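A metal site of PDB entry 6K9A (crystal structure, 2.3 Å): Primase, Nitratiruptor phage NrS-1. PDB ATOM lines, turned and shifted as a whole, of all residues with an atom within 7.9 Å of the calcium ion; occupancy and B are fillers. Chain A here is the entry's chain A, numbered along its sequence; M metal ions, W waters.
The side-chain carboxylate of Glu 143 lies within salt-bridge range of the side-chain amino group of Lys 122 (2.7 Å).
The side-chain carboxylate of Asp 73 lies close to the side-chain amide oxygen of Gln 17, at 3.1 Å.
Four residues have an atom within 4 Å of the calcium ion: Thr 70, Asp 73, Phe 75 and Glu 143.
The calcium ion is bound by water W1, O of Glu 143, OD1 of Asp 73, O of Thr 70 and O of Phe 75.
Slightly farther from the calcium ion lies O of Asp 73 (2.9 Å).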
ATOM      1  N   GLN A  17      16.537  -9.646  -1.242  1.00  0.00           N
ATOM      2  CA  GLN A  17      15.206  -9.061  -1.356  1.00  0.00           C
ATOM      3  C   GLN A  17      14.837  -8.324  -0.079  1.00  0.00           C
ATOM      4  O   GLN A  17      13.677  -8.299   0.337  1.00  0.00           O
ATOM      5  CB  GLN A  17      14.163 -10.139  -1.665  1.00  0.00           C
ATOM      6  CG  GLN A  17      14.448 -10.932  -2.931  1.00  0.00           C
ATOM      7  CD  GLN A  17      13.537 -12.132  -3.088  1.00  0.00           C
ATOM      8  OE1 GLN A  17      12.589 -12.320  -2.311  1.00  0.00           O
ATOM      9  NE2 GLN A  17      13.812 -12.961  -4.086  1.00  0.00           N
ATOM     10  N   PHE A  67      11.224  -7.621   3.989  1.00  0.00           N
ATOM     11  CA  PHE A  67      11.552  -8.627   2.985  1.00  0.00           C
ATOM     12  C   PHE A  67      10.489  -8.583   1.888  1.00  0.00           C
ATOM     13  O   PHE A  67       9.299  -8.663   2.182  1.00  0.00           O
ATOM     14  CB  PHE A  67      11.639 -10.024   3.597  1.00  0.00           C
ATOM     15  CG  PHE A  67      12.232 -11.056   2.678  1.00  0.00           C
ATOM     16  CD1 PHE A  67      11.426 -11.800   1.831  1.00  0.00           C
ATOM     17  CD2 PHE A  67      13.596 -11.279   2.673  1.00  0.00           C
ATOM     18  CE1 PHE A  67      11.972 -12.741   0.988  1.00  0.00           C
ATOM     19  CE2 PHE A  67      14.149 -12.229   1.822  1.00  0.00           C
ATOM     20  CZ  PHE A  67      13.337 -12.963   0.984  1.00  0.00           C
ATOM     21  N   VAL A  68      10.937  -8.475   0.640  1.00  0.00           N
ATOM     22  CA  VAL A  68      10.033  -8.381  -0.499  1.00  0.00           C
ATOM     23  C   VAL A  68       9.742  -9.785  -1.014  1.00  0.00           C
ATOM     24  O   VAL A  68      10.674 -10.532  -1.353  1.00  0.00           O
ATOM     25  CB  VAL A  68      10.612  -7.497  -1.609  1.00  0.00           C
ATOM     26  CG1 VAL A  68       9.618  -7.378  -2.751  1.00  0.00           C
ATOM     27  CG2 VAL A  68      10.984  -6.134  -1.066  1.00  0.00           C
ATOM     28  N   LEU A  69       8.462 -10.141  -1.085  1.00  0.00           N
ATOM     29  CA  LEU A  69       8.074 -11.435  -1.623  1.00  0.00           C
ATOM     30  C   LEU A  69       7.890 -11.324  -3.127  1.00  0.00           C
ATOM     31  O   LEU A  69       7.254 -10.392  -3.619  1.00  0.00           O
ATOM     32  CB  LEU A  69       6.790 -11.928  -0.966  1.00  0.00           C
ATOM     33  CG  LEU A  69       6.848 -12.144   0.548  1.00  0.00           C
ATOM     34  CD1 LEU A  69       6.118 -11.029   1.282  1.00  0.00           C
ATOM     35  CD2 LEU A  69       6.292 -13.506   0.918  1.00  0.00           C
ATOM     36  N   THR A  70       8.466 -12.285  -3.858  1.00  0.00           N
ATOM     37  CA  THR A  70       8.302 -12.381  -5.300  1.00  0.00           C
ATOM     38  C   THR A  70       7.695 -13.736  -5.633  1.00  0.00           C
ATOM     39  O   THR A  70       7.728 -14.677  -4.827  1.00  0.00           O
ATOM     40  CB  THR A  70       9.634 -12.204  -6.037  1.00  0.00           C
ATOM     41  OG1 THR A  70      10.511 -13.292  -5.721  1.00  0.00           O
ATOM     42  CG2 THR A  70      10.301 -10.901  -5.619  1.00  0.00           C
ATOM     43  N   LYS A  71       7.122 -13.831  -6.837  1.00  0.00           N
ATOM     44  CA  LYS A  71       6.497 -15.072  -7.271  1.00  0.00           C
ATOM     45  C   LYS A  71       7.508 -16.170  -7.563  1.00  0.00           C
ATOM     46  O   LYS A  71       7.105 -17.328  -7.743  1.00  0.00           O
ATOM     47  CB  LYS A  71       5.643 -14.797  -8.510  1.00  0.00           C
ATOM     48  CG  LYS A  71       6.189 -13.705  -9.410  1.00  0.00           C
ATOM     49  CD  LYS A  71       5.089 -13.011 -10.194  1.00  0.00           C
ATOM     50  CE  LYS A  71       5.610 -11.740 -10.869  1.00  0.00           C
ATOM     51  NZ  LYS A  71       6.874 -11.989 -11.627  1.00  0.00           N
ATOM     52  N   SER A  72       8.798 -15.858  -7.593  1.00  0.00           N
ATOM     53  CA  SER A  72       9.822 -16.857  -7.882  1.00  0.00           C
ATOM     54  C   SER A  72      10.435 -17.475  -6.630  1.00  0.00           C
ATOM     55  O   SER A  72      10.894 -18.616  -6.676  1.00  0.00           O
ATOM     56  CB  SER A  72      10.929 -16.246  -8.747  1.00  0.00           C
ATOM     57  OG  SER A  72      10.378 -15.405  -9.755  1.00  0.00           O
ATOM     58  N   ASP A  73      10.456 -16.748  -5.520  1.00  0.00           N
ATOM     59  CA  ASP A  73      10.910 -17.335  -4.260  1.00  0.00           C
ATOM     60  C   ASP A  73       9.802 -18.222  -3.687  1.00  0.00           C
ATOM     61  O   ASP A  73       8.635 -18.095  -4.065  1.00  0.00           O
ATOM     62  CB  ASP A  73      11.304 -16.231  -3.271  1.00  0.00           C
ATOM     63  CG  ASP A  73      10.180 -15.257  -2.985  1.00  0.00           C
ATOM     64  OD1 ASP A  73       9.199 -15.657  -2.329  1.00  0.00           O
ATOM     65  OD2 ASP A  73      10.296 -14.084  -3.401  1.00  0.00           O
ATOM     66  N   PRO A  74      10.149 -19.130  -2.777  1.00  0.00           N
ATOM     67  CA  PRO A  74       9.140 -20.074  -2.266  1.00  0.00           C
ATOM     68  C   PRO A  74       8.329 -19.589  -1.074  1.00  0.00           C
ATOM     69  O   PRO A  74       7.585 -20.394  -0.500  1.00  0.00           O
ATOM     70  CB  PRO A  74      10.000 -21.291  -1.848  1.00  0.00           C
ATOM     71  CG  PRO A  74      11.461 -20.852  -1.989  1.00  0.00           C
ATOM     72  CD  PRO A  74      11.466 -19.381  -2.169  1.00  0.00           C
ATOM     73  N   PHE A  75       8.411 -18.316  -0.709  1.00  0.00           N
ATOM     74  CA  PHE A  75       7.877 -17.845   0.563  1.00  0.00           C
ATOM     75  C   PHE A  75       6.447 -17.346   0.422  1.00  0.00           C
ATOM     76  O   PHE A  75       6.107 -16.641  -0.539  1.00  0.00           O
ATOM     77  CB  PHE A  75       8.752 -16.744   1.130  1.00  0.00           C
ATOM     78  CG  PHE A  75      10.194 -17.137   1.267  1.00  0.00           C
ATOM     79  CD1 PHE A  75      11.156 -16.603   0.436  1.00  0.00           C
ATOM     80  CD2 PHE A  75      10.574 -18.076   2.215  1.00  0.00           C
ATOM     81  CE1 PHE A  75      12.483 -16.977   0.556  1.00  0.00           C
ATOM     82  CE2 PHE A  75      11.892 -18.454   2.344  1.00  0.00           C
ATOM     83  CZ  PHE A  75      12.847 -17.904   1.514  1.00  0.00           C
ATOM     84  N   VAL A  76       5.605 -17.712   1.385  1.00  0.00           N
ATOM     85  CA  VAL A  76       4.245 -17.207   1.504  1.00  0.00           C
ATOM     86  C   VAL A  76       4.133 -16.416   2.801  1.00  0.00           C
ATOM     87  O   VAL A  76       4.578 -16.889   3.856  1.00  0.00           O
ATOM     88  CB  VAL A  76       3.197 -18.344   1.470  1.00  0.00           C
ATOM     89  CG1 VAL A  76       1.812 -17.791   1.759  1.00  0.00           C
ATOM     90  CG2 VAL A  76       3.222 -19.046   0.120  1.00  0.00           C
ATOM     91  N   PHE A  77       3.551 -15.225   2.712  1.00  0.00           N
ATOM     92  CA  PHE A  77       3.409 -14.324   3.855  1.00  0.00           C
ATOM     93  C   PHE A  77       1.965 -14.380   4.346  1.00  0.00           C
ATOM     94  O   PHE A  77       1.038 -14.034   3.608  1.00  0.00           O
ATOM     95  CB  PHE A  77       3.805 -12.899   3.453  1.00  0.00           C
ATOM     96  CG  PHE A  77       3.472 -11.845   4.483  1.00  0.00           C
ATOM     97  CD1 PHE A  77       3.054 -10.583   4.072  1.00  0.00           C
ATOM     98  CD2 PHE A  77       3.569 -12.111   5.839  1.00  0.00           C
ATOM     99  CE1 PHE A  77       2.755  -9.613   5.006  1.00  0.00           C
ATOM    100  CE2 PHE A  77       3.257 -11.146   6.769  1.00  0.00           C
ATOM    101  CZ  PHE A  77       2.848  -9.886   6.355  1.00  0.00           C
ATOM    102  N   VAL A 119       5.656 -19.275   5.339  1.00  0.00           N
ATOM    103  CA  VAL A 119       5.628 -20.674   4.920  1.00  0.00           C
ATOM    104  C   VAL A 119       6.300 -20.762   3.554  1.00  0.00           C
ATOM    105  O   VAL A 119       6.261 -19.818   2.764  1.00  0.00           O
ATOM    106  CB  VAL A 119       4.190 -21.230   4.860  1.00  0.00           C
ATOM    107  CG1 VAL A 119       4.176 -22.712   4.489  1.00  0.00           C
ATOM    108  CG2 VAL A 119       3.476 -21.008   6.182  1.00  0.00           C
ATOM    109  N   SER A 120       6.917 -21.911   3.288  1.00  0.00           N
ATOM    110  CA  SER A 120       7.383 -22.247   1.948  1.00  0.00           C
ATOM    111  C   SER A 120       6.274 -23.049   1.259  1.00  0.00           C
ATOM    112  O   SER A 120       5.985 -24.177   1.655  1.00  0.00           O
ATOM    113  CB  SER A 120       8.685 -23.038   1.998  1.00  0.00           C
ATOM    114  OG  SER A 120       9.150 -23.324   0.698  1.00  0.00           O
ATOM    115  N   GLY A 121       5.656 -22.457   0.244  1.00  0.00           N
ATOM    116  CA  GLY A 121       4.590 -23.141  -0.465  1.00  0.00           C
ATOM    117  C   GLY A 121       3.895 -22.224  -1.445  1.00  0.00           C
ATOM    118  O   GLY A 121       4.482 -21.255  -1.943  1.00  0.00           O
ATOM    119  N   LYS A 122       2.636 -22.553  -1.727  1.00  0.00           N
ATOM    120  CA  LYS A 122       1.837 -21.857  -2.715  1.00  0.00           C
ATOM    121  C   LYS A 122       0.435 -21.632  -2.177  1.00  0.00           C
ATOM    122  O   LYS A 122      -0.163 -22.526  -1.565  1.00  0.00           O
ATOM    123  CB  LYS A 122       1.765 -22.665  -4.018  1.00  0.00           C
ATOM    124  CG  LYS A 122       0.852 -22.073  -5.087  1.00  0.00           C
ATOM    125  CD  LYS A 122       1.453 -20.825  -5.706  1.00  0.00           C
ATOM    126  CE  LYS A 122       0.442 -20.085  -6.559  1.00  0.00           C
ATOM    127  NZ  LYS A 122      -0.679 -19.543  -5.735  1.00  0.00           N
ATOM    128  N   TYR A 142      -0.230 -13.124   1.146  1.00  0.00           N
ATOM    129  CA  TYR A 142       0.405 -12.741  -0.104  1.00  0.00           C
ATOM    130  C   TYR A 142       1.652 -13.588  -0.291  1.00  0.00           C
ATOM    131  O   TYR A 142       2.305 -13.982   0.678  1.00  0.00           O
ATOM    132  CB  TYR A 142       0.791 -11.252  -0.143  1.00  0.00           C
ATOM    133  CG  TYR A 142      -0.389 -10.304  -0.083  1.00  0.00           C
ATOM    134  CD1 TYR A 142      -1.150 -10.041  -1.219  1.00  0.00           C
ATOM    135  CD2 TYR A 142      -0.728  -9.658   1.092  1.00  0.00           C
ATOM    136  CE1 TYR A 142      -2.224  -9.166  -1.171  1.00  0.00           C
ATOM    137  CE2 TYR A 142      -1.798  -8.782   1.154  1.00  0.00           C
ATOM    138  CZ  TYR A 142      -2.542  -8.544   0.023  1.00  0.00           C
ATOM    139  OH  TYR A 142      -3.606  -7.677   0.077  1.00  0.00           O
ATOM    140  N   GLU A 143       1.969 -13.877  -1.548  1.00  0.00           N
ATOM    141  CA  GLU A 143       3.187 -14.588  -1.908  1.00  0.00           C
ATOM    142  C   GLU A 143       4.053 -13.815  -2.888  1.00  0.00           C
ATOM    143  O   GLU A 143       5.150 -14.266  -3.210  1.00  0.00           O
ATOM    144  CB  GLU A 143       2.847 -15.968  -2.478  1.00  0.00           C
ATOM    145  CG  GLU A 143       2.119 -15.919  -3.817  1.00  0.00           C
ATOM    146  CD  GLU A 143       1.419 -17.233  -4.139  1.00  0.00           C
ATOM    147  OE1 GLU A 143       0.373 -17.191  -4.824  1.00  0.00           O
ATOM    148  OE2 GLU A 143       1.909 -18.289  -3.704  1.00  0.00           O
ATOM    149  N   SER A 144       3.590 -12.652  -3.353  1.00  0.00           N
ATOM    150  CA  SER A 144       4.332 -11.852  -4.305  1.00  0.00           C
ATOM    151  C   SER A 144       3.734 -10.455  -4.341  1.00  0.00           C
ATOM    152  O   SER A 144       2.663 -10.200  -3.804  1.00  0.00           O
ATOM    153  CB  SER A 144       4.310 -12.478  -5.708  1.00  0.00           C
ATOM    154  OG  SER A 144       4.667 -11.535  -6.696  1.00  0.00           O
ATOM    155  N   GLY A 145       4.467  -9.540  -4.979  1.00  0.00           N
ATOM    156  CA  GLY A 145       3.975  -8.199  -5.233  1.00  0.00           C
ATOM    157  C   GLY A 145       3.968  -7.260  -4.039  1.00  0.00           C
ATOM    158  O   GLY A 145       3.551  -6.110  -4.193  1.00  0.00           O
HETATM  159 CA    CA M   1       6.792 -16.128  -2.964  1.00  0.00          CA
HETATM  160  O   HOH W   1       6.069 -17.685  -4.698  1.00  0.00           O
